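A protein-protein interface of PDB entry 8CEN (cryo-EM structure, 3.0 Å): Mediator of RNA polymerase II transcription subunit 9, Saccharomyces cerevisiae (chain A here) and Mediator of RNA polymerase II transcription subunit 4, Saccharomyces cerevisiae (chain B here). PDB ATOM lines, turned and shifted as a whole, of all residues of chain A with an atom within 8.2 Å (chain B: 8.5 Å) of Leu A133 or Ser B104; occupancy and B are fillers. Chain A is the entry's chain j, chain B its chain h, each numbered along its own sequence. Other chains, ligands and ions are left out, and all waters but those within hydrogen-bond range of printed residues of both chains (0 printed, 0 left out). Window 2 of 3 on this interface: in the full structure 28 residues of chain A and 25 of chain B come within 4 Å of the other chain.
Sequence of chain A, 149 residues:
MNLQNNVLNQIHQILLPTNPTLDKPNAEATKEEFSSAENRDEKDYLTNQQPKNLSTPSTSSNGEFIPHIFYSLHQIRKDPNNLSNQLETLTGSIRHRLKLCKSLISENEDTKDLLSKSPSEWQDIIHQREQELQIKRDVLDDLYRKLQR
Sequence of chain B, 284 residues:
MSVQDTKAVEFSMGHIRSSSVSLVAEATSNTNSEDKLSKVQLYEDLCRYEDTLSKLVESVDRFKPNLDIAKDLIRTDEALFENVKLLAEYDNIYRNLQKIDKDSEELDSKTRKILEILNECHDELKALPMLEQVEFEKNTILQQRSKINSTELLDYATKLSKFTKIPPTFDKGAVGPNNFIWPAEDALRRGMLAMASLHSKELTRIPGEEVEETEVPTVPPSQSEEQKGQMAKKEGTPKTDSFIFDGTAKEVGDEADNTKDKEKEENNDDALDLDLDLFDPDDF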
ATOM      1  N   ILE A 126     -16.848  33.793  13.667  1.00  0.00           N
ATOM      2  CA  ILE A 126     -17.263  32.654  14.478  1.00  0.00           C
ATOM      3  C   ILE A 126     -17.780  31.528  13.579  1.00  0.00           C
ATOM      4  O   ILE A 126     -17.540  30.343  13.863  1.00  0.00           O
ATOM      5  CB  ILE A 126     -18.277  33.088  15.562  1.00  0.00           C
ATOM      6  CG1 ILE A 126     -18.512  31.972  16.571  1.00  0.00           C
ATOM      7  CG2 ILE A 126     -19.623  33.493  14.991  1.00  0.00           C
ATOM      8  CD1 ILE A 126     -19.237  32.442  17.818  1.00  0.00           C
ATOM      9  N   GLN A 128     -16.578  30.925  10.562  1.00  0.00           N
ATOM     10  CA  GLN A 128     -15.385  30.357   9.945  1.00  0.00           C
ATOM     11  C   GLN A 128     -14.434  29.724  10.951  1.00  0.00           C
ATOM     12  O   GLN A 128     -13.471  29.071  10.538  1.00  0.00           O
ATOM     13  CB  GLN A 128     -14.625  31.416   9.126  1.00  0.00           C
ATOM     14  CG  GLN A 128     -13.770  32.395   9.936  1.00  0.00           C
ATOM     15  CD  GLN A 128     -12.301  31.989  10.027  1.00  0.00           C
ATOM     16  OE1 GLN A 128     -11.751  31.391   9.102  1.00  0.00           O
ATOM     17  NE2 GLN A 128     -11.667  32.308  11.151  1.00  0.00           N
ATOM     18  N   ARG A 129     -14.655  29.917  12.252  1.00  0.00           N
ATOM     19  CA  ARG A 129     -13.875  29.201  13.250  1.00  0.00           C
ATOM     20  C   ARG A 129     -14.612  27.973  13.787  1.00  0.00           C
ATOM     21  O   ARG A 129     -13.981  27.105  14.401  1.00  0.00           O
ATOM     22  CB  ARG A 129     -13.461  30.193  14.361  1.00  0.00           C
ATOM     23  CG  ARG A 129     -12.465  29.724  15.431  1.00  0.00           C
ATOM     24  CD  ARG A 129     -13.074  29.112  16.680  1.00  0.00           C
ATOM     25  NE  ARG A 129     -13.916  30.067  17.388  1.00  0.00           N
ATOM     26  CZ  ARG A 129     -14.800  29.742  18.319  1.00  0.00           C
ATOM     27  NH1 ARG A 129     -15.000  28.483  18.672  1.00  0.00           N
ATOM     28  NH2 ARG A 129     -15.490  30.706  18.923  1.00  0.00           N
ATOM     29  N   GLU A 130     -15.919  27.849  13.509  1.00  0.00           N
ATOM     30  CA  GLU A 130     -16.665  26.649  13.903  1.00  0.00           C
ATOM     31  C   GLU A 130     -16.200  25.376  13.188  1.00  0.00           C
ATOM     32  O   GLU A 130     -16.166  24.301  13.805  1.00  0.00           O
ATOM     33  CB  GLU A 130     -18.161  26.868  13.659  1.00  0.00           C
ATOM     34  CG  GLU A 130     -19.059  25.741  14.165  1.00  0.00           C
ATOM     35  CD  GLU A 130     -19.133  25.669  15.675  1.00  0.00           C
ATOM     36  OE1 GLU A 130     -18.943  26.712  16.332  1.00  0.00           O
ATOM     37  OE2 GLU A 130     -19.372  24.562  16.205  1.00  0.00           O
ATOM     38  N   GLN A 131     -15.847  25.451  11.898  1.00  0.00           N
ATOM     39  CA  GLN A 131     -15.536  24.214  11.178  1.00  0.00           C
ATOM     40  C   GLN A 131     -14.186  23.635  11.581  1.00  0.00           C
ATOM     41  O   GLN A 131     -13.929  22.454  11.330  1.00  0.00           O
ATOM     42  CB  GLN A 131     -15.592  24.410   9.658  1.00  0.00           C
ATOM     43  CG  GLN A 131     -14.494  25.269   9.053  1.00  0.00           C
ATOM     44  CD  GLN A 131     -14.828  26.738   9.115  1.00  0.00           C
ATOM     45  OE1 GLN A 131     -15.713  27.146   9.858  1.00  0.00           O
ATOM     46  NE2 GLN A 131     -14.127  27.545   8.331  1.00  0.00           N
ATOM     47  N   GLU A 132     -13.316  24.431  12.206  1.00  0.00           N
ATOM     48  CA  GLU A 132     -12.121  23.856  12.816  1.00  0.00           C
ATOM     49  C   GLU A 132     -12.486  22.937  13.978  1.00  0.00           C
ATOM     50  O   GLU A 132     -11.919  21.848  14.122  1.00  0.00           O
ATOM     51  CB  GLU A 132     -11.175  24.967  13.274  1.00  0.00           C
ATOM     52  CG  GLU A 132     -10.479  25.725  12.142  1.00  0.00           C
ATOM     53  CD  GLU A 132      -9.278  24.985  11.558  1.00  0.00           C
ATOM     54  OE1 GLU A 132      -9.424  23.837  11.088  1.00  0.00           O
ATOM     55  OE2 GLU A 132      -8.173  25.566  11.569  1.00  0.00           O
ATOM     56  N   LEU A 133     -13.459  23.339  14.798  1.00  0.00           N
ATOM     57  CA  LEU A 133     -13.957  22.433  15.824  1.00  0.00           C
ATOM     58  C   LEU A 133     -14.702  21.255  15.213  1.00  0.00           C
ATOM     59  O   LEU A 133     -14.700  20.159  15.782  1.00  0.00           O
ATOM     60  CB  LEU A 133     -14.857  23.181  16.802  1.00  0.00           C
ATOM     61  CG  LEU A 133     -14.106  24.229  17.616  1.00  0.00           C
ATOM     62  CD1 LEU A 133     -15.061  25.040  18.482  1.00  0.00           C
ATOM     63  CD2 LEU A 133     -13.025  23.556  18.438  1.00  0.00           C
ATOM     64  N   GLN A 134     -15.342  21.465  14.061  1.00  0.00           N
ATOM     65  CA  GLN A 134     -15.998  20.357  13.371  1.00  0.00           C
ATOM     66  C   GLN A 134     -14.986  19.319  12.890  1.00  0.00           C
ATOM     67  O   GLN A 134     -15.219  18.109  13.020  1.00  0.00           O
ATOM     68  CB  GLN A 134     -16.831  20.882  12.202  1.00  0.00           C
ATOM     69  CG  GLN A 134     -17.871  19.901  11.684  1.00  0.00           C
ATOM     70  CD  GLN A 134     -17.345  19.035  10.557  1.00  0.00           C
ATOM     71  OE1 GLN A 134     -16.478  19.455   9.789  1.00  0.00           O
ATOM     72  NE2 GLN A 134     -17.867  17.819  10.452  1.00  0.00           N
ATOM     73  N   ILE A 135     -13.854  19.769  12.342  1.00  0.00           N
ATOM     74  CA  ILE A 135     -12.829  18.821  11.915  1.00  0.00           C
ATOM     75  C   ILE A 135     -12.148  18.194  13.132  1.00  0.00           C
ATOM     76  O   ILE A 135     -11.729  17.032  13.081  1.00  0.00           O
ATOM     77  CB  ILE A 135     -11.827  19.482  10.936  1.00  0.00           C
ATOM     78  CG1 ILE A 135     -11.194  18.436  10.014  1.00  0.00           C
ATOM     79  CG2 ILE A 135     -10.711  20.236  11.639  1.00  0.00           C
ATOM     80  CD1 ILE A 135     -12.124  17.929   8.941  1.00  0.00           C
ATOM     81  N   LYS A 136     -12.071  18.920  14.256  1.00  0.00           N
ATOM     82  CA  LYS A 136     -11.570  18.304  15.483  1.00  0.00           C
ATOM     83  C   LYS A 136     -12.498  17.193  15.957  1.00  0.00           C
ATOM     84  O   LYS A 136     -12.033  16.110  16.331  1.00  0.00           O
ATOM     85  CB  LYS A 136     -11.382  19.355  16.576  1.00  0.00           C
ATOM     86  CG  LYS A 136     -10.142  20.212  16.398  1.00  0.00           C
ATOM     87  CD  LYS A 136     -10.055  21.298  17.457  1.00  0.00           C
ATOM     88  CE  LYS A 136      -8.736  22.047  17.359  1.00  0.00           C
ATOM     89  NZ  LYS A 136      -8.616  22.786  16.073  1.00  0.00           N
ATOM     90  N   ARG A 137     -13.813  17.421  15.900  1.00  0.00           N
ATOM     91  CA  ARG A 137     -14.761  16.378  16.281  1.00  0.00           C
ATOM     92  C   ARG A 137     -14.722  15.191  15.321  1.00  0.00           C
ATOM     93  O   ARG A 137     -14.860  14.041  15.754  1.00  0.00           O
ATOM     94  CB  ARG A 137     -16.185  16.934  16.384  1.00  0.00           C
ATOM     95  CG  ARG A 137     -16.547  17.434  17.781  1.00  0.00           C
ATOM     96  CD  ARG A 137     -17.634  18.510  17.807  1.00  0.00           C
ATOM     97  NE  ARG A 137     -17.311  19.749  17.111  1.00  0.00           N
ATOM     98  CZ  ARG A 137     -18.181  20.439  16.383  1.00  0.00           C
ATOM     99  NH1 ARG A 137     -19.411  19.997  16.175  1.00  0.00           N
ATOM    100  NH2 ARG A 137     -17.815  21.608  15.868  1.00  0.00           N
ATOM    101  N   ASP A 138     -14.546  15.432  14.016  1.00  0.00           N
ATOM    102  CA  ASP A 138     -14.608  14.282  13.115  1.00  0.00           C
ATOM    103  C   ASP A 138     -13.307  13.465  13.113  1.00  0.00           C
ATOM    104  O   ASP A 138     -13.360  12.228  13.052  1.00  0.00           O
ATOM    105  CB  ASP A 138     -15.119  14.705  11.716  1.00  0.00           C
ATOM    106  CG  ASP A 138     -14.088  15.400  10.817  1.00  0.00           C
ATOM    107  OD1 ASP A 138     -12.885  15.489  11.098  1.00  0.00           O
ATOM    108  OD2 ASP A 138     -14.533  15.877   9.752  1.00  0.00           O
ATOM    109  N   VAL A 139     -12.141  14.109  13.256  1.00  0.00           N
ATOM    110  CA  VAL A 139     -10.919  13.347  13.524  1.00  0.00           C
ATOM    111  C   VAL A 139     -10.879  12.841  14.968  1.00  0.00           C
ATOM    112  O   VAL A 139     -10.031  12.012  15.319  1.00  0.00           O
ATOM    113  CB  VAL A 139      -9.676  14.195  13.147  1.00  0.00           C
ATOM    114  CG1 VAL A 139      -8.399  13.364  13.099  1.00  0.00           C
ATOM    115  CG2 VAL A 139      -9.846  14.801  11.776  1.00  0.00           C
ATOM    116  N   LEU A 140     -11.801  13.288  15.822  1.00  0.00           N
ATOM    117  CA  LEU A 140     -11.933  12.658  17.128  1.00  0.00           C
ATOM    118  C   LEU A 140     -12.727  11.357  17.037  1.00  0.00           C
ATOM    119  O   LEU A 140     -12.314  10.333  17.593  1.00  0.00           O
ATOM    120  CB  LEU A 140     -12.577  13.644  18.113  1.00  0.00           C
ATOM    121  CG  LEU A 140     -12.707  13.365  19.617  1.00  0.00           C
ATOM    122  CD1 LEU A 140     -12.738  14.690  20.356  1.00  0.00           C
ATOM    123  CD2 LEU A 140     -13.961  12.574  19.971  1.00  0.00           C
ATOM    124  N   LEU B  97     -20.385  32.661  21.878  1.00  0.00           N
ATOM    125  CA  LEU B  97     -18.953  32.468  21.684  1.00  0.00           C
ATOM    126  C   LEU B  97     -18.317  31.838  22.914  1.00  0.00           C
ATOM    127  O   LEU B  97     -17.425  30.998  22.791  1.00  0.00           O
ATOM    128  CB  LEU B  97     -18.290  33.810  21.344  1.00  0.00           C
ATOM    129  CG  LEU B  97     -16.832  33.891  20.874  1.00  0.00           C
ATOM    130  CD1 LEU B  97     -16.672  35.070  19.931  1.00  0.00           C
ATOM    131  CD2 LEU B  97     -15.847  34.036  22.030  1.00  0.00           C
ATOM    132  N   GLN B  98     -18.765  32.232  24.110  1.00  0.00           N
ATOM    133  CA  GLN B  98     -18.284  31.602  25.337  1.00  0.00           C
ATOM    134  C   GLN B  98     -18.717  30.143  25.422  1.00  0.00           C
ATOM    135  O   GLN B  98     -17.953  29.294  25.894  1.00  0.00           O
ATOM    136  CB  GLN B  98     -18.785  32.379  26.556  1.00  0.00           C
ATOM    137  CG  GLN B  98     -18.015  32.095  27.839  1.00  0.00           C
ATOM    138  CD  GLN B  98     -16.602  32.646  27.813  1.00  0.00           C
ATOM    139  OE1 GLN B  98     -16.383  33.832  28.063  1.00  0.00           O
ATOM    140  NE2 GLN B  98     -15.635  31.787  27.512  1.00  0.00           N
ATOM    141  N   LYS B  99     -19.941  29.839  24.973  1.00  0.00           N
ATOM    142  CA  LYS B  99     -20.421  28.458  24.963  1.00  0.00           C
ATOM    143  C   LYS B  99     -19.557  27.570  24.070  1.00  0.00           C
ATOM    144  O   LYS B  99     -19.139  26.474  24.471  1.00  0.00           O
ATOM    145  CB  LYS B  99     -21.881  28.419  24.508  1.00  0.00           C
ATOM    146  CG  LYS B  99     -22.401  27.021  24.213  1.00  0.00           C
ATOM    147  CD  LYS B  99     -23.558  27.055  23.229  1.00  0.00           C
ATOM    148  CE  LYS B  99     -24.774  27.740  23.832  1.00  0.00           C
ATOM    149  NZ  LYS B  99     -25.404  26.915  24.902  1.00  0.00           N
ATOM    150  N   ILE B 100     -19.255  28.031  22.856  1.00  0.00           N
ATOM    151  CA  ILE B 100     -18.424  27.174  22.012  1.00  0.00           C
ATOM    152  C   ILE B 100     -16.940  27.283  22.368  1.00  0.00           C
ATOM    153  O   ILE B 100     -16.173  26.366  22.068  1.00  0.00           O
ATOM    154  CB  ILE B 100     -18.673  27.431  20.518  1.00  0.00           C
ATOM    155  CG1 ILE B 100     -18.259  28.834  20.104  1.00  0.00           C
ATOM    156  CG2 ILE B 100     -20.141  27.192  20.186  1.00  0.00           C
ATOM    157  CD1 ILE B 100     -18.313  28.996  18.618  1.00  0.00           C
ATOM    158  N   ASP B 101     -16.515  28.343  23.057  1.00  0.00           N
ATOM    159  CA  ASP B 101     -15.167  28.351  23.617  1.00  0.00           C
ATOM    160  C   ASP B 101     -15.028  27.286  24.699  1.00  0.00           C
ATOM    161  O   ASP B 101     -14.012  26.580  24.764  1.00  0.00           O
ATOM    162  CB  ASP B 101     -14.839  29.741  24.164  1.00  0.00           C
ATOM    163  CG  ASP B 101     -13.353  29.949  24.393  1.00  0.00           C
ATOM    164  OD1 ASP B 101     -12.786  29.318  25.310  1.00  0.00           O
ATOM    165  OD2 ASP B 101     -12.747  30.747  23.648  1.00  0.00           O
ATOM    166  N   LYS B 102     -16.058  27.130  25.540  1.00  0.00           N
ATOM    167  CA  LYS B 102     -15.969  26.120  26.586  1.00  0.00           C
ATOM    168  C   LYS B 102     -16.124  24.709  26.021  1.00  0.00           C
ATOM    169  O   LYS B 102     -15.476  23.781  26.524  1.00  0.00           O
ATOM    170  CB  LYS B 102     -16.980  26.388  27.711  1.00  0.00           C
ATOM    171  CG  LYS B 102     -18.402  25.902  27.499  1.00  0.00           C
ATOM    172  CD  LYS B 102     -19.232  26.053  28.761  1.00  0.00           C
ATOM    173  CE  LYS B 102     -20.601  25.412  28.596  1.00  0.00           C
ATOM    174  NZ  LYS B 102     -21.477  26.191  27.679  1.00  0.00           N
ATOM    175  N   ASP B 103     -16.922  24.514  24.957  1.00  0.00           N
ATOM    176  CA  ASP B 103     -16.960  23.145  24.443  1.00  0.00           C
ATOM    177  C   ASP B 103     -15.693  22.826  23.648  1.00  0.00           C
ATOM    178  O   ASP B 103     -15.249  21.669  23.642  1.00  0.00           O
ATOM    179  CB  ASP B 103     -18.277  22.843  23.685  1.00  0.00           C
ATOM    180  CG  ASP B 103     -18.382  23.436  22.268  1.00  0.00           C
ATOM    181  OD1 ASP B 103     -17.460  24.047  21.715  1.00  0.00           O
ATOM    182  OD2 ASP B 103     -19.471  23.267  21.682  1.00  0.00           O
ATOM    183  N   SER B 104     -15.060  23.847  23.053  1.00  0.00           N
ATOM    184  CA  SER B 104     -13.733  23.684  22.465  1.00  0.00           C
ATOM    185  C   SER B 104     -12.698  23.279  23.507  1.00  0.00           C
ATOM    186  O   SER B 104     -11.902  22.357  23.276  1.00  0.00           O
ATOM    187  CB  SER B 104     -13.307  24.985  21.788  1.00  0.00           C
ATOM    188  OG  SER B 104     -12.015  24.867  21.223  1.00  0.00           O
ATOM    189  N   GLU B 105     -12.684  23.954  24.659  1.00  0.00           N
ATOM    190  CA  GLU B 105     -11.661  23.622  25.645  1.00  0.00           C
ATOM    191  C   GLU B 105     -11.931  22.274  26.305  1.00  0.00           C
ATOM    192  O   GLU B 105     -10.980  21.552  26.626  1.00  0.00           O
ATOM    193  CB  GLU B 105     -11.510  24.739  26.688  1.00  0.00           C
ATOM    194  CG  GLU B 105     -12.683  24.973  27.619  1.00  0.00           C
ATOM    195  CD  GLU B 105     -12.609  24.143  28.889  1.00  0.00           C
ATOM    196  OE1 GLU B 105     -11.505  23.663  29.224  1.00  0.00           O
ATOM    197  OE2 GLU B 105     -13.656  23.967  29.547  1.00  0.00           O
ATOM    198  N   GLU B 106     -13.202  21.882  26.477  1.00  0.00           N
ATOM    199  CA  GLU B 106     -13.433  20.560  27.054  1.00  0.00           C
ATOM    200  C   GLU B 106     -13.158  19.452  26.043  1.00  0.00           C
ATOM    201  O   GLU B 106     -12.735  18.361  26.438  1.00  0.00           O
ATOM    202  CB  GLU B 106     -14.848  20.430  27.636  1.00  0.00           C
ATOM    203  CG  GLU B 106     -16.009  20.531  26.666  1.00  0.00           C
ATOM    204  CD  GLU B 106     -16.386  19.204  26.026  1.00  0.00           C
ATOM    205  OE1 GLU B 106     -16.021  18.148  26.583  1.00  0.00           O
ATOM    206  OE2 GLU B 106     -17.044  19.221  24.964  1.00  0.00           O
ATOM    207  N   LEU B 107     -13.356  19.701  24.740  1.00  0.00           N
ATOM    208  CA  LEU B 107     -12.962  18.677  23.774  1.00  0.00           C
ATOM    209  C   LEU B 107     -11.445  18.578  23.664  1.00  0.00           C
ATOM    210  O   LEU B 107     -10.913  17.478  23.481  1.00  0.00           O
ATOM    211  CB  LEU B 107     -13.610  18.932  22.405  1.00  0.00           C
ATOM    212  CG  LEU B 107     -13.237  20.053  21.428  1.00  0.00           C
ATOM    213  CD1 LEU B 107     -12.118  19.648  20.470  1.00  0.00           C
ATOM    214  CD2 LEU B 107     -14.464  20.488  20.641  1.00  0.00           C
ATOM    215  N   ASP B 108     -10.733  19.703  23.799  1.00  0.00           N
ATOM    216  CA  ASP B 108      -9.273  19.648  23.858  1.00  0.00           C
ATOM    217  C   ASP B 108      -8.795  18.891  25.095  1.00  0.00           C
ATOM    218  O   ASP B 108      -7.833  18.110  25.028  1.00  0.00           O
ATOM    219  CB  ASP B 108      -8.694  21.062  23.829  1.00  0.00           C
ATOM    220  CG  ASP B 108      -8.618  21.631  22.424  1.00  0.00           C
ATOM    221  OD1 ASP B 108      -8.749  20.849  21.458  1.00  0.00           O
ATOM    222  OD2 ASP B 108      -8.430  22.857  22.285  1.00  0.00           O
ATOM    223  N   SER B 109      -9.464  19.107  26.234  1.00  0.00           N
ATOM    224  CA  SER B 109      -9.148  18.361  27.448  1.00  0.00           C
ATOM    225  C   SER B 109      -9.419  16.871  27.269  1.00  0.00           C
ATOM    226  O   SER B 109      -8.637  16.031  27.733  1.00  0.00           O
ATOM    227  CB  SER B 109      -9.950  18.916  28.625  1.00  0.00           C
ATOM    228  OG  SER B 109      -9.720  20.304  28.787  1.00  0.00           O
ATOM    229  N   LYS B 110     -10.521  16.532  26.594  1.00  0.00           N
ATOM    230  CA  LYS B 110     -10.831  15.135  26.303  1.00  0.00           C
ATOM    231  C   LYS B 110      -9.756  14.500  25.429  1.00  0.00           C
ATOM    232  O   LYS B 110      -9.327  13.370  25.689  1.00  0.00           O
ATOM    233  CB  LYS B 110     -12.197  15.031  25.623  1.00  0.00           C
ATOM    234  CG  LYS B 110     -12.611  13.611  25.267  1.00  0.00           C
ATOM    235  CD  LYS B 110     -13.967  13.583  24.577  1.00  0.00           C
ATOM    236  CE  LYS B 110     -15.103  13.654  25.581  1.00  0.00           C
ATOM    237  NZ  LYS B 110     -15.310  12.351  26.267  1.00  0.00           N
ATOM    238  N   THR B 111      -9.303  15.221  24.396  1.00  0.00           N
ATOM    239  CA  THR B 111      -8.260  14.691  23.521  1.00  0.00           C
ATOM    240  C   THR B 111      -6.952  14.473  24.270  1.00  0.00           C
ATOM    241  O   THR B 111      -6.308  13.430  24.107  1.00  0.00           O
ATOM    242  CB  THR B 111      -8.032  15.615  22.323  1.00  0.00           C
ATOM    243  OG1 THR B 111      -7.726  16.938  22.781  1.00  0.00           O
ATOM    244  CG2 THR B 111      -9.248  15.635  21.408  1.00  0.00           C
ATOM    245  N   ARG B 112      -6.550  15.428  25.116  1.00  0.00           N
ATOM    246  CA  ARG B 112      -5.278  15.247  25.810  1.00  0.00           C
ATOM    247  C   ARG B 112      -5.362  14.157  26.878  1.00  0.00           C
ATOM    248  O   ARG B 112      -4.391  13.411  27.072  1.00  0.00           O
ATOM    249  CB  ARG B 112      -4.778  16.572  26.396  1.00  0.00           C
ATOM    250  CG  ARG B 112      -5.652  17.230  27.442  1.00  0.00           C
ATOM    251  CD  ARG B 112      -4.997  18.501  27.967  1.00  0.00           C
ATOM    252  NE  ARG B 112      -4.646  19.417  26.887  1.00  0.00           N
ATOM    253  CZ  ARG B 112      -5.432  20.383  26.434  1.00  0.00           C
ATOM    254  NH1 ARG B 112      -6.629  20.602  26.954  1.00  0.00           N
ATOM    255  NH2 ARG B 112      -5.006  21.152  25.436  1.00  0.00           N
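OG1 of Thr B111 sits at hydrogen-bond distance from O of Asp B108, 2.5 Å away. O of Leu A133 is in hydrogen-bond range of NE of Arg A137 (3.0 Å). The guanidinium group (NH2) of Arg A137 is in salt-bridge range of the side-chain carboxylate (OE2) of Glu A130 (3.4 Å). The backbone carbonyl oxygen (O) of Leu B107 lies close to the side-chain hydroxyl (OG1) of Thr B111 (3.3 Å). The side-chain carboxylate (OD1) of Asp B103 lies close to the backbone carbonyl oxygen (O) of Ile B100, at 2.7 Å.
Among the printed residues, merely in contact across the chains: Leu A133 with Ser B104 (3.2 Å), Glu A130 with Ile B100 (3.3 Å), Arg A129 with Ile B100 (3.3 Å), Ile A126 with Ile B100 (3.6 Å), Leu A140 with Thr B111 (3.8 Å), Ile A126 with Leu B97 (3.9 Å), Arg A129 with Leu B97 (3.97 Å), Lys A136 with Leu B107 (3.97 Å) and Leu A133 with Ile B100 (3.98 Å).
Of the printed residues of chain B, Ile A126 touches Leu B97 (3.9 Å) and Ile B100 (3.6 Å). Printed residues of chain B within 4 Å of Glu A130: Ile B100 (3.3 Å). Printed residues of chain B within 4 Å of Leu A133: Ile B100 and Ser B104. Printed residues of chain B within 4 Å of Lys A136: Leu B107. Arg A137 touches none of the printed residues of chain B. Of the printed residues of chain B, Leu A140 touches Thr B111 (3.8 Å). Printed residues of chain A within 4 Å of Leu B97: Ile A126 and Arg A129. Ser B104 touches one residue of chain A. Glu B106 touches none of the printed residues of chain A.
Of the 16 printed residues of chain B, 5 touch a printed residue of chain A. Printed residues of chain B that touch a printed residue of chain A: Leu B97, Ile B100, Ser B104, Leu B107 and Thr B111. Of the 14 printed residues of chain A, 6 touch a printed residue of chain B. Hydrophobic or aromatic side chains of chain A within 4 Å of the printed part of chain B: Ile A126, Leu A133 and Leu A140. Among the printed residues, 9 pairs touch across the chains. Among the printed residues, no Asp or Glu carboxylate lies within 4 Å of a Lys or Arg side-chain nitrogen of the other chain.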
